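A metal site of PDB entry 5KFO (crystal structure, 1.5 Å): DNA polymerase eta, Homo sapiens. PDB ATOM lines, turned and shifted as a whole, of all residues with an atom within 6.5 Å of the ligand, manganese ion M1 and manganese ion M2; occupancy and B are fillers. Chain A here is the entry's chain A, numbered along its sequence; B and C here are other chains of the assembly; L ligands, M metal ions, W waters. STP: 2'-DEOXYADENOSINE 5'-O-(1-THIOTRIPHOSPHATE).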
ATOM      1  N   ASP A  16      23.449  31.490  11.324  1.00  0.00           N
ATOM      2  CA  ASP A  16      22.518  30.398  11.632  1.00  0.00           C
ATOM      3  C   ASP A  16      23.054  29.560  12.786  1.00  0.00           C
ATOM      4  O   ASP A  16      24.166  29.050  12.704  1.00  0.00           O
ATOM      5  CB  ASP A  16      22.305  29.528  10.403  1.00  0.00           C
ATOM      6  CG  ASP A  16      21.302  28.452  10.641  1.00  0.00           C
ATOM      7  OD1 ASP A  16      21.678  27.423  11.209  1.00  0.00           O
ATOM      8  OD2 ASP A  16      20.127  28.653  10.263  1.00  0.00           O
ATOM      9  N   MET A  17      22.272  29.389  13.850  1.00  0.00           N
ATOM     10  CA  MET A  17      22.764  28.664  15.010  1.00  0.00           C
ATOM     11  C   MET A  17      23.027  27.193  14.715  1.00  0.00           C
ATOM     12  O   MET A  17      22.305  26.592  13.932  1.00  0.00           O
ATOM     13  CB  MET A  17      21.769  28.789  16.174  1.00  0.00           C
ATOM     14  CG  MET A  17      21.351  30.207  16.484  1.00  0.00           C
ATOM     15  SD  MET A  17      22.726  31.324  16.841  1.00  0.00           S
ATOM     16  CE  MET A  17      23.428  30.577  18.279  1.00  0.00           C
ATOM     17  N   ASP A  18      24.050  26.618  15.326  1.00  0.00           N
ATOM     18  CA  ASP A  18      24.326  25.181  15.132  1.00  0.00           C
ATOM     19  C   ASP A  18      23.384  24.371  16.003  1.00  0.00           C
ATOM     20  O   ASP A  18      23.192  24.719  17.167  1.00  0.00           O
ATOM     21  CB  ASP A  18      25.781  24.864  15.466  1.00  0.00           C
ATOM     22  CG  ASP A  18      26.778  25.600  14.577  1.00  0.00           C
ATOM     23  OD1 ASP A  18      26.446  25.924  13.413  1.00  0.00           O
ATOM     24  OD2 ASP A  18      27.897  25.842  15.052  1.00  0.00           O
ATOM     25  N   CYS A  19      22.806  23.329  15.404  1.00  0.00           N
ATOM     26  CA  CYS A  19      21.858  22.427  16.067  1.00  0.00           C
ATOM     27  C   CYS A  19      21.134  23.125  17.223  1.00  0.00           C
ATOM     28  O   CYS A  19      21.281  22.751  18.391  1.00  0.00           O
ATOM     29  CB  CYS A  19      22.574  21.132  16.535  1.00  0.00           C
ATOM     30  SG  CYS A  19      24.052  21.260  17.557  1.00  0.00           S
ATOM     31  N   PHE A  20      20.369  24.155  16.895  1.00  0.00           N
ATOM     32  CA  PHE A  20      19.959  25.156  17.875  1.00  0.00           C
ATOM     33  C   PHE A  20      19.228  24.617  19.107  1.00  0.00           C
ATOM     34  O   PHE A  20      19.661  24.885  20.223  1.00  0.00           O
ATOM     35  CB  PHE A  20      19.070  26.217  17.211  1.00  0.00           C
ATOM     36  CG  PHE A  20      18.738  27.369  18.117  1.00  0.00           C
ATOM     37  CD1 PHE A  20      19.734  27.925  18.915  1.00  0.00           C
ATOM     38  CD2 PHE A  20      17.457  27.894  18.178  1.00  0.00           C
ATOM     39  CE1 PHE A  20      19.448  29.006  19.773  1.00  0.00           C
ATOM     40  CE2 PHE A  20      17.159  28.981  19.038  1.00  0.00           C
ATOM     41  CZ  PHE A  20      18.161  29.521  19.821  1.00  0.00           C
ATOM     42  N   PHE A  21      18.142  23.887  18.914  1.00  0.00           N
ATOM     43  CA  PHE A  21      17.392  23.460  20.101  1.00  0.00           C
ATOM     44  C   PHE A  21      18.257  22.554  20.987  1.00  0.00           C
ATOM     45  O   PHE A  21      18.114  22.536  22.216  1.00  0.00           O
ATOM     46  CB  PHE A  21      16.097  22.716  19.734  1.00  0.00           C
ATOM     47  CG  PHE A  21      15.005  23.588  19.143  1.00  0.00           C
ATOM     48  CD1 PHE A  21      15.251  24.882  18.696  1.00  0.00           C
ATOM     49  CD2 PHE A  21      13.732  23.082  19.022  1.00  0.00           C
ATOM     50  CE1 PHE A  21      14.207  25.654  18.132  1.00  0.00           C
ATOM     51  CE2 PHE A  21      12.700  23.843  18.477  1.00  0.00           C
ATOM     52  CZ  PHE A  21      12.939  25.125  18.026  1.00  0.00           C
ATOM     53  N   VAL A  22      19.128  21.756  20.355  1.00  0.00           N
ATOM     54  CA  VAL A  22      20.047  20.916  21.126  1.00  0.00           C
ATOM     55  C   VAL A  22      20.987  21.790  21.960  1.00  0.00           C
ATOM     56  O   VAL A  22      21.187  21.515  23.143  1.00  0.00           O
ATOM     57  CB  VAL A  22      20.847  19.994  20.194  1.00  0.00           C
ATOM     58  CG1 VAL A  22      22.054  19.393  20.937  1.00  0.00           C
ATOM     59  CG2 VAL A  22      19.951  18.888  19.624  1.00  0.00           C
ATOM     60  N   GLN A  41       9.838  15.733  20.389  1.00  0.00           N
ATOM     61  CA  GLN A  41       8.494  16.200  20.744  1.00  0.00           C
ATOM     62  C   GLN A  41       7.605  14.993  20.962  1.00  0.00           C
ATOM     63  O   GLN A  41       7.547  14.115  20.105  1.00  0.00           O
ATOM     64  CB  GLN A  41       7.894  17.061  19.635  1.00  0.00           C
ATOM     65  CG  GLN A  41       8.081  18.538  19.787  1.00  0.00           C
ATOM     66  CD  GLN A  41       7.645  19.308  18.557  1.00  0.00           C
ATOM     67  OE1 GLN A  41       7.464  18.746  17.476  1.00  0.00           O
ATOM     68  NE2 GLN A  41       7.455  20.608  18.719  1.00  0.00           N
ATOM     69  N   ILE A  51      13.370  16.672  16.411  1.00  0.00           N
ATOM     70  CA  ILE A  51      13.341  17.928  15.670  1.00  0.00           C
ATOM     71  C   ILE A  51      14.696  18.641  15.617  1.00  0.00           C
ATOM     72  O   ILE A  51      14.862  19.597  14.858  1.00  0.00           O
ATOM     73  CB  ILE A  51      12.270  18.894  16.235  1.00  0.00           C
ATOM     74  CG1 ILE A  51      12.525  19.223  17.713  1.00  0.00           C
ATOM     75  CG2 ILE A  51      10.872  18.307  16.019  1.00  0.00           C
ATOM     76  CD1 ILE A  51      11.574  20.324  18.233  1.00  0.00           C
ATOM     77  N   ALA A  52      15.672  18.174  16.388  1.00  0.00           N
ATOM     78  CA  ALA A  52      17.029  18.738  16.330  1.00  0.00           C
ATOM     79  C   ALA A  52      18.026  17.670  16.767  1.00  0.00           C
ATOM     80  O   ALA A  52      17.700  16.832  17.625  1.00  0.00           O
ATOM     81  CB  ALA A  52      17.159  20.000  17.211  1.00  0.00           C
ATOM     82  N   VAL A  53      19.225  17.699  16.172  1.00  0.00           N
ATOM     83  CA  VAL A  53      20.201  16.618  16.318  1.00  0.00           C
ATOM     84  C   VAL A  53      21.611  17.177  16.486  1.00  0.00           C
ATOM     85  O   VAL A  53      22.059  17.954  15.637  1.00  0.00           O
ATOM     86  CB  VAL A  53      20.198  15.680  15.066  1.00  0.00           C
ATOM     87  CG1 VAL A  53      21.064  14.445  15.305  1.00  0.00           C
ATOM     88  CG2 VAL A  53      18.788  15.247  14.733  1.00  0.00           C
ATOM     89  N   TYR A  55      25.734  17.254  16.387  1.00  0.00           N
ATOM     90  CA  TYR A  55      26.604  16.773  15.329  1.00  0.00           C
ATOM     91  C   TYR A  55      27.197  15.411  15.644  1.00  0.00           C
ATOM     92  O   TYR A  55      27.386  14.604  14.727  1.00  0.00           O
ATOM     93  CB  TYR A  55      27.699  17.811  15.011  1.00  0.00           C
ATOM     94  CG  TYR A  55      27.136  18.898  14.134  1.00  0.00           C
ATOM     95  CD1 TYR A  55      26.373  19.925  14.671  1.00  0.00           C
ATOM     96  CD2 TYR A  55      27.272  18.842  12.753  1.00  0.00           C
ATOM     97  CE1 TYR A  55      25.806  20.891  13.887  1.00  0.00           C
ATOM     98  CE2 TYR A  55      26.706  19.815  11.941  1.00  0.00           C
ATOM     99  CZ  TYR A  55      25.974  20.835  12.507  1.00  0.00           C
ATOM    100  OH  TYR A  55      25.406  21.803  11.714  1.00  0.00           O
ATOM    101  N   ARG A  58      24.487  13.108  14.512  1.00  0.00           N
ATOM    102  CA  ARG A  58      24.406  13.035  13.050  1.00  0.00           C
ATOM    103  C   ARG A  58      25.405  12.043  12.455  1.00  0.00           C
ATOM    104  O   ARG A  58      25.129  11.431  11.412  1.00  0.00           O
ATOM    105  CB  ARG A  58      24.625  14.407  12.425  1.00  0.00           C
ATOM    106  CG  ARG A  58      23.632  15.419  12.901  1.00  0.00           C
ATOM    107  CD  ARG A  58      23.806  16.751  12.204  1.00  0.00           C
ATOM    108  NE  ARG A  58      23.028  17.778  12.904  1.00  0.00           N
ATOM    109  CZ  ARG A  58      22.785  18.995  12.447  1.00  0.00           C
ATOM    110  NH1 ARG A  58      23.240  19.362  11.250  1.00  0.00           N
ATOM    111  NH2 ARG A  58      22.065  19.845  13.198  1.00  0.00           N
ATOM    112  N   ARG A  64      16.573  14.822  11.685  1.00  0.00           N
ATOM    113  CA  ARG A  64      15.249  15.368  11.915  1.00  0.00           C
ATOM    114  C   ARG A  64      14.189  14.492  11.243  1.00  0.00           C
ATOM    115  O   ARG A  64      14.460  13.864  10.229  1.00  0.00           O
ATOM    116  CB  ARG A  64      15.205  16.811  11.405  1.00  0.00           C
ATOM    117  CG  ARG A  64      13.839  17.436  11.386  1.00  0.00           C
ATOM    118  CD  ARG A  64      13.940  18.891  10.975  1.00  0.00           C
ATOM    119  NE  ARG A  64      14.805  19.603  11.891  1.00  0.00           N
ATOM    120  CZ  ARG A  64      15.931  20.228  11.544  1.00  0.00           C
ATOM    121  NH1 ARG A  64      16.315  20.257  10.271  1.00  0.00           N
ATOM    122  NH2 ARG A  64      16.635  20.840  12.483  1.00  0.00           N
ATOM    123  N   LEU A  92       7.027  25.768  22.622  1.00  0.00           N
ATOM    124  CA  LEU A  92       8.382  26.119  22.150  1.00  0.00           C
ATOM    125  C   LEU A  92       8.955  27.374  22.792  1.00  0.00           C
ATOM    126  O   LEU A  92       9.951  27.917  22.299  1.00  0.00           O
ATOM    127  CB  LEU A  92       8.365  26.276  20.623  1.00  0.00           C
ATOM    128  CG  LEU A  92       7.795  25.087  19.843  1.00  0.00           C
ATOM    129  CD1 LEU A  92       7.740  25.397  18.342  1.00  0.00           C
ATOM    130  CD2 LEU A  92       8.657  23.851  20.123  1.00  0.00           C
ATOM    131  N   SER A 116      14.241  32.988  10.682  1.00  0.00           N
ATOM    132  CA  SER A 116      13.669  31.809  11.337  1.00  0.00           C
ATOM    133  C   SER A 116      13.909  31.934  12.836  1.00  0.00           C
ATOM    134  O   SER A 116      14.490  32.903  13.294  1.00  0.00           O
ATOM    135  CB  SER A 116      14.288  30.512  10.834  1.00  0.00           C
ATOM    136  OG  SER A 116      15.578  30.318  11.422  1.00  0.00           O
ATOM    137  N   ILE A 117      13.523  30.908  13.594  1.00  0.00           N
ATOM    138  CA  ILE A 117      13.784  30.950  15.022  1.00  0.00           C
ATOM    139  C   ILE A 117      15.295  30.949  15.322  1.00  0.00           C
ATOM    140  O   ILE A 117      15.720  31.366  16.392  1.00  0.00           O
ATOM    141  CB  ILE A 117      13.094  29.762  15.734  1.00  0.00           C
ATOM    142  CG1 ILE A 117      12.980  30.021  17.238  1.00  0.00           C
ATOM    143  CG2 ILE A 117      13.830  28.459  15.458  1.00  0.00           C
ATOM    144  CD1 ILE A 117      12.048  29.018  17.938  1.00  0.00           C
ATOM    145  N   ASP A 118      16.117  30.492  14.371  1.00  0.00           N
ATOM    146  CA  ASP A 118      17.545  30.374  14.692  1.00  0.00           C
ATOM    147  C   ASP A 118      18.483  31.067  13.678  1.00  0.00           C
ATOM    148  O   ASP A 118      19.694  30.795  13.678  1.00  0.00           O
ATOM    149  CB  ASP A 118      17.957  28.897  14.841  1.00  0.00           C
ATOM    150  CG  ASP A 118      18.451  28.279  13.545  1.00  0.00           C
ATOM    151  OD1 ASP A 118      17.869  28.508  12.446  1.00  0.00           O
ATOM    152  OD2 ASP A 118      19.508  27.612  13.640  1.00  0.00           O
ATOM    153  N   GLU A 119      17.962  31.962  12.847  1.00  0.00           N
ATOM    154  CA  GLU A 119      18.851  32.652  11.914  1.00  0.00           C
ATOM    155  C   GLU A 119      18.364  34.005  11.506  1.00  0.00           C
ATOM    156  O   GLU A 119      17.150  34.283  11.518  1.00  0.00           O
ATOM    157  CB  GLU A 119      19.092  31.813  10.661  1.00  0.00           C
ATOM    158  CG  GLU A 119      17.916  31.777   9.700  1.00  0.00           C
ATOM    159  CD  GLU A 119      17.881  30.477   8.925  1.00  0.00           C
ATOM    160  OE1 GLU A 119      18.363  30.455   7.775  1.00  0.00           O
ATOM    161  OE2 GLU A 119      17.392  29.477   9.481  1.00  0.00           O
ATOM    162  N   SER A 216      27.139  29.200  12.795  1.00  0.00           N
ATOM    163  CA  SER A 216      27.885  29.336  11.557  1.00  0.00           C
ATOM    164  C   SER A 216      27.393  30.560  10.829  1.00  0.00           C
ATOM    165  O   SER A 216      26.381  31.138  11.207  1.00  0.00           O
ATOM    166  CB  SER A 216      27.708  28.087  10.698  1.00  0.00           C
ATOM    167  OG  SER A 216      28.215  26.962  11.390  1.00  0.00           O
ATOM    168  N   LYS A 227      23.191  32.656   2.540  1.00  0.00           N
ATOM    169  CA  LYS A 227      22.585  31.450   3.084  1.00  0.00           C
ATOM    170  C   LYS A 227      23.306  30.193   2.593  1.00  0.00           C
ATOM    171  O   LYS A 227      23.609  29.274   3.372  1.00  0.00           O
ATOM    172  CB  LYS A 227      21.089  31.385   2.717  1.00  0.00           C
ATOM    173  CG  LYS A 227      20.388  30.104   3.178  1.00  0.00           C
ATOM    174  CD  LYS A 227      20.389  29.932   4.702  1.00  0.00           C
ATOM    175  CE  LYS A 227      19.579  28.690   5.079  1.00  0.00           C
ATOM    176  NZ  LYS A 227      19.596  28.375   6.547  1.00  0.00           N
ATOM    177  N   LYS A 234      29.585  24.327   8.131  1.00  0.00           N
ATOM    178  CA  LYS A 234      29.019  24.015   9.442  1.00  0.00           C
ATOM    179  C   LYS A 234      29.632  22.766  10.074  1.00  0.00           C
ATOM    180  O   LYS A 234      29.967  21.827   9.365  1.00  0.00           O
ATOM    181  CB  LYS A 234      27.500  23.804   9.337  1.00  0.00           C
ATOM    182  CG  LYS A 234      26.655  25.054   9.380  1.00  0.00           C
ATOM    183  CD  LYS A 234      25.175  24.735   9.641  1.00  0.00           C
ATOM    184  CE  LYS A 234      24.379  25.982  10.076  1.00  0.00           C
ATOM    185  NZ  LYS A 234      24.280  26.119  11.571  1.00  0.00           N
ATOM    186  N   PRO A 235      29.763  22.745  11.411  1.00  0.00           N
ATOM    187  CA  PRO A 235      29.358  23.778  12.358  1.00  0.00           C
ATOM    188  C   PRO A 235      30.513  24.644  12.834  1.00  0.00           C
ATOM    189  O   PRO A 235      31.682  24.346  12.579  1.00  0.00           O
ATOM    190  CB  PRO A 235      28.820  22.958  13.535  1.00  0.00           C
ATOM    191  CG  PRO A 235      29.772  21.777  13.573  1.00  0.00           C
ATOM    192  CD  PRO A 235      30.167  21.510  12.114  1.00  0.00           C
ATOM    193  P    DT B   8      15.472  28.635   4.843  1.00  0.00           P
ATOM    194  OP1  DT B   8      15.937  30.020   4.669  1.00  0.00           O
ATOM    195  OP2  DT B   8      16.196  27.523   4.202  1.00  0.00           O
ATOM    196  O5'  DT B   8      15.453  28.448   6.403  1.00  0.00           O
ATOM    197  C5'  DT B   8      15.004  27.294   6.892  1.00  0.00           C
ATOM    198  C4'  DT B   8      14.648  27.438   8.331  1.00  0.00           C
ATOM    199  O4'  DT B   8      13.257  27.077   8.439  1.00  0.00           O
ATOM    200  C3'  DT B   8      15.435  26.452   9.176  1.00  0.00           C
ATOM    201  O3'  DT B   8      15.971  27.062  10.348  1.00  0.00           O
ATOM    202  C2'  DT B   8      14.440  25.329   9.485  1.00  0.00           C
ATOM    203  C1'  DT B   8      13.093  26.026   9.371  1.00  0.00           C
ATOM    204  N1   DT B   8      12.026  25.116   8.876  1.00  0.00           N
ATOM    205  C2   DT B   8      10.927  24.898   9.674  1.00  0.00           C
ATOM    206  O2   DT B   8      10.806  25.415  10.768  1.00  0.00           O
ATOM    207  N3   DT B   8       9.989  24.058   9.148  1.00  0.00           N
ATOM    208  C4   DT B   8      10.031  23.415   7.939  1.00  0.00           C
ATOM    209  O4   DT B   8       9.129  22.659   7.558  1.00  0.00           O
ATOM    210  C5   DT B   8      11.202  23.677   7.143  1.00  0.00           C
ATOM    211  C7   DT B   8      11.344  23.025   5.790  1.00  0.00           C
ATOM    212  C6   DT B   8      12.134  24.511   7.637  1.00  0.00           C
ATOM    213  P    DT C   3       4.440   9.543   9.338  1.00  0.00           P
ATOM    214  OP1  DT C   3       3.507   9.631   8.186  1.00  0.00           O
ATOM    215  OP2  DT C   3       5.419   8.437   9.415  1.00  0.00           O
ATOM    216  O5'  DT C   3       5.236  10.924   9.439  1.00  0.00           O
ATOM    217  C5'  DT C   3       6.030  11.203  10.586  1.00  0.00           C
ATOM    218  C4'  DT C   3       6.470  12.657  10.583  1.00  0.00           C
ATOM    219  O4'  DT C   3       7.514  12.838   9.599  1.00  0.00           O
ATOM    220  C3'  DT C   3       5.365  13.642  10.216  1.00  0.00           C
ATOM    221  O3'  DT C   3       5.054  14.481  11.333  1.00  0.00           O
ATOM    222  C2'  DT C   3       5.910  14.446   9.025  1.00  0.00           C
ATOM    223  C1'  DT C   3       7.388  14.094   9.000  1.00  0.00           C
ATOM    224  N1   DT C   3       7.939  14.020   7.613  1.00  0.00           N
ATOM    225  C2   DT C   3       8.932  14.891   7.232  1.00  0.00           C
ATOM    226  O2   DT C   3       9.398  15.735   7.965  1.00  0.00           O
ATOM    227  N3   DT C   3       9.365  14.725   5.943  1.00  0.00           N
ATOM    228  C4   DT C   3       8.908  13.801   5.015  1.00  0.00           C
ATOM    229  O4   DT C   3       9.360  13.735   3.875  1.00  0.00           O
ATOM    230  C5   DT C   3       7.869  12.916   5.485  1.00  0.00           C
ATOM    231  C7   DT C   3       7.299  11.876   4.577  1.00  0.00           C
ATOM    232  C6   DT C   3       7.433  13.066   6.749  1.00  0.00           C
ATOM    233  P    DT C   4       2.254  14.153  12.841  1.00  0.00           P
ATOM    234  OP1  DT C   4       1.514  13.446  13.907  1.00  0.00           O
ATOM    235  OP2  DT C   4       1.567  14.635  11.626  1.00  0.00           O
ATOM    236  O5'  DT C   4       2.948  15.422  13.498  1.00  0.00           O
ATOM    237  C5'  DT C   4       3.857  15.234  14.543  1.00  0.00           C
ATOM    238  C4'  DT C   4       4.221  16.567  15.169  1.00  0.00           C
ATOM    239  O4'  DT C   4       5.354  17.162  14.505  1.00  0.00           O
ATOM    240  C3'  DT C   4       3.141  17.631  15.181  1.00  0.00           C
ATOM    241  O3'  DT C   4       3.181  18.304  16.420  1.00  0.00           O
ATOM    242  C2'  DT C   4       3.553  18.558  14.018  1.00  0.00           C
ATOM    243  C1'  DT C   4       5.055  18.496  14.159  1.00  0.00           C
ATOM    244  N1   DT C   4       5.827  18.785  12.949  1.00  0.00           N
ATOM    245  C2   DT C   4       7.004  19.462  13.121  1.00  0.00           C
ATOM    246  O2   DT C   4       7.362  19.887  14.202  1.00  0.00           O
ATOM    247  N3   DT C   4       7.718  19.642  11.975  1.00  0.00           N
ATOM    248  C4   DT C   4       7.410  19.213  10.708  1.00  0.00           C
ATOM    249  O4   DT C   4       8.142  19.450   9.752  1.00  0.00           O
ATOM    250  C5   DT C   4       6.174  18.469  10.601  1.00  0.00           C
ATOM    251  C7   DT C   4       5.713  17.945   9.256  1.00  0.00           C
ATOM    252  C6   DT C   4       5.453  18.282  11.724  1.00  0.00           C
ATOM    253  P    DA C   5       2.169  19.495  16.754  1.00  0.00           P
ATOM    254  OP1  DA C   5       1.797  19.378  18.181  1.00  0.00           O
ATOM    255  OP2  DA C   5       1.140  19.561  15.698  1.00  0.00           O
ATOM    256  O5'  DA C   5       3.048  20.798  16.570  1.00  0.00           O
ATOM    257  C5'  DA C   5       4.119  21.060  17.482  1.00  0.00           C
ATOM    258  C4'  DA C   5       4.710  22.419  17.181  1.00  0.00           C
ATOM    259  O4'  DA C   5       5.433  22.361  15.915  1.00  0.00           O
ATOM    260  C3'  DA C   5       3.688  23.549  17.036  1.00  0.00           C
ATOM    261  O3'  DA C   5       4.213  24.739  17.620  1.00  0.00           O
ATOM    262  C2'  DA C   5       3.547  23.695  15.524  1.00  0.00           C
ATOM    263  C1'  DA C   5       4.982  23.405  15.092  1.00  0.00           C
ATOM    264  N9   DA C   5       5.124  22.975  13.711  1.00  0.00           N
ATOM    265  C8   DA C   5       4.261  22.194  12.995  1.00  0.00           C
ATOM    266  N7   DA C   5       4.658  21.945  11.778  1.00  0.00           N
ATOM    267  C5   DA C   5       5.873  22.614  11.680  1.00  0.00           C
ATOM    268  C6   DA C   5       6.801  22.752  10.632  1.00  0.00           C
ATOM    269  N6   DA C   5       6.640  22.193   9.429  1.00  0.00           N
ATOM    270  N1   DA C   5       7.904  23.477  10.866  1.00  0.00           N
ATOM    271  C2   DA C   5       8.062  24.043  12.080  1.00  0.00           C
ATOM    272  N3   DA C   5       7.266  23.987  13.141  1.00  0.00           N
ATOM    273  C4   DA C   5       6.172  23.243  12.862  1.00  0.00           C
HETATM  274  PG  STP L   1      22.112  23.143  11.809  1.00  0.00           P
HETATM  275  O1G STP L   1      21.651  24.478  11.511  1.00  0.00           O
HETATM  276  O2G STP L   1      23.346  23.224  12.567  1.00  0.00           O
HETATM  277  O3G STP L   1      22.187  22.194  10.659  1.00  0.00           O
HETATM  278  PB  STP L   1      19.710  23.182  13.395  1.00  0.00           P
HETATM  279  O1B STP L   1      19.966  24.495  14.003  1.00  0.00           O
HETATM  280  O2B STP L   1      19.071  22.298  14.389  1.00  0.00           O
HETATM  281  O3B STP L   1      21.062  22.541  12.833  1.00  0.00           O
HETATM  282  PA  STP L   1      17.964  24.424  11.470  1.00  0.00           P
HETATM  283  S1A STP L   1      17.398  23.667   9.746  1.00  0.00           S
HETATM  284  O2A STP L   1      18.692  25.687  11.344  1.00  0.00           O
HETATM  285  O3A STP L   1      18.784  23.218  12.107  1.00  0.00           O
HETATM  286  O5' STP L   1      16.739  24.640  12.352  1.00  0.00           O
HETATM  287  C5' STP L   1      16.805  25.405  13.470  1.00  0.00           C
HETATM  288  C4' STP L   1      15.917  24.891  14.611  1.00  0.00           C
HETATM  289  O4' STP L   1      14.603  24.944  14.174  1.00  0.00           O
HETATM  290  C3' STP L   1      16.129  23.501  14.942  1.00  0.00           C
HETATM  291  O3' STP L   1      17.067  23.293  15.972  1.00  0.00           O
HETATM  292  C2' STP L   1      14.832  23.004  15.379  1.00  0.00           C
HETATM  293  C1' STP L   1      13.890  23.770  14.528  1.00  0.00           C
HETATM  294  N9  STP L   1      13.397  23.122  13.348  1.00  0.00           N
HETATM  295  C8  STP L   1      13.970  23.054  12.148  1.00  0.00           C
HETATM  296  N7  STP L   1      13.235  22.410  11.304  1.00  0.00           N
HETATM  297  C5  STP L   1      12.157  22.013  11.883  1.00  0.00           C
HETATM  298  C6  STP L   1      10.976  21.296  11.557  1.00  0.00           C
HETATM  299  N6  STP L   1      10.838  20.833  10.255  1.00  0.00           N
HETATM  300  N1  STP L   1      10.020  21.081  12.483  1.00  0.00           N
HETATM  301  C2  STP L   1      10.107  21.514  13.756  1.00  0.00           C
HETATM  302  N3  STP L   1      11.217  22.216  14.097  1.00  0.00           N
HETATM  303  C4  STP L   1      12.233  22.459  13.221  1.00  0.00           C
HETATM  304 MN    MN M   1      20.660  26.173  12.599  1.00  0.00          MN
HETATM  305 MN    MN M   2      18.201  27.706  10.442  1.00  0.00          MN
HETATM  306  O   HOH W   1      21.160  25.177   8.757  1.00  0.00           O
HETATM  307  O   HOH W   2      11.367  25.977  13.381  1.00  0.00           O
HETATM  308  O   HOH W   3      13.578  21.587   8.594  1.00  0.00           O
HETATM  309  O   HOH W   4      18.753  26.509   8.674  1.00  0.00           O
HETATM  310  O   HOH W   5      19.303  19.594  14.076  1.00  0.00           O
HETATM  311  O   HOH W   6      14.290  27.015  12.217  1.00  0.00           O
HETATM  312  O   HOH W   7      19.925  20.708   9.770  1.00  0.00           O
HETATM  313  O   HOH W   8      10.101  23.533  16.366  1.00  0.00           O
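A nitrogen (N6) of the ligand lies within hydrogen-bond range of O4 of DT 4 of chain C. NH1 of Arg 58 lies within salt-bridge range of O3G of the ligand (3.1 Å). The backbone NH (N) of Phe 21 sits at hydrogen-bond distance from an oxygen (O3') of the ligand (3.2 Å). An oxygen (O2G) of the ligand lies within hydrogen-bond range of the backbone NH of Cys 19 (2.9 Å). The side-chain amino group of Lys 234 is in salt-bridge range of an oxygen (O2G) of the ligand, at 3.2 Å. N of Phe 20 lies within hydrogen-bond range of O2B of the ligand (3.4 Å). OH of Tyr 55 is in hydrogen-bond range of O2G of the ligand, 2.6 Å away. The guanidinium group (NH2) of Arg 64 is in salt-bridge range of an oxygen (O2B) of the ligand (3.4 Å).
The side-chain amino group (NZ) of Lys 234 is in salt-bridge range of the side-chain carboxylate (OD1) of Asp 18, at 2.9 Å. N of Glu 119 sits at hydrogen-bond distance from OG of Ser 116 (3.2 Å). The backbone carbonyl oxygen (O) of Met 17 sits close to the side-chain amino group (NZ) of Lys 234. The side-chain amino group (NZ) of Lys 227 is in salt-bridge range of the side-chain carboxylate (OE1) of Glu 119 (2.7 Å). The side-chain carboxylate (OD2) of Asp 16 sits close to the side-chain amino group (NZ) of Lys 227, 3.8 Å away. N of Asp 118 lies within hydrogen-bond range of OG of Ser 116 (3.0 Å). The backbone carbonyl oxygen (O) of Asp 16 sits at hydrogen-bond distance from the side-chain amino group (NZ) of Lys 234. O2 of DT 4 of chain C sits close to OE1 of Gln 41.
Merely in contact with the ligand: Asp 18 (3.4 Å), Ile 51 (3.4 Å), Ala 52 (3.5 Å), DA 5 of chain C (3.6 Å) and Ile 117 (3.8 Å). Hydrophobic or aromatic side chains that line the ligand: Phe 20, Phe 21, Ile 51, Ala 52, Tyr 55 and Ile 117. 17 residues have an atom within 4 Å of the ligand: Asp 16, Met 17, Asp 18, Cys 19, Phe 20, Phe 21, Ile 51, Ala 52, Tyr 55, Arg 58, Arg 64, Ile 117, Asp 118, Lys 234, DT 8 of chain B, DT 4 of chain C and DA 5 of chain C. Along chain A the residues within 4 Å of the ligand span positions 16 to 234.
NZ of Lys 234 touches manganese ion M1, 3.8 Å away. The nearest printed residue that does not touch manganese ion M1 is Asp 18 (4.4 Å).
OG of Ser 116 touches manganese ion M2, 3.8 Å away. Within 4 Å of manganese ion M2: Asp 16, Ser 116, Asp 118, Glu 119 and DT 8 of chain B.
The side-chain carboxylate (OD2) of Asp 118 binds manganese ion M1 (2.1 Å). OD1 of Asp 16 binds manganese ion M1 (2.1 Å). O of Met 17 is bound to manganese ion M1, at 2.2 Å. Manganese ion M1 is bound by O1G of the ligand (2.2 Å). An oxygen (O1B) of the ligand is bound to manganese ion M1, 2.3 Å away. Manganese ion M1 is bound by an oxygen (O2A) of the ligand (2.4 Å). Manganese ion M1 has six donor atoms within binding distance.
Manganese ion M2 is bound by OD2 of Asp 16, OE2 of Glu 119, OD1 of Asp 118, water W4, O2A of the ligand and O3' of DT 8 of chain B.
Water W4 bridges the side-chain amino group of Lys 227 and a sulfur (S1A) of the ligand. Water W3 lies within hydrogen-bond range of N7 of the ligand (2.9 Å) and NH1 of Arg 64 (3.5 Å). Water W2 bridges O2 of DT 8 of chain B (2.7 Å) and an oxygen (O4') of the ligand (3.5 Å).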
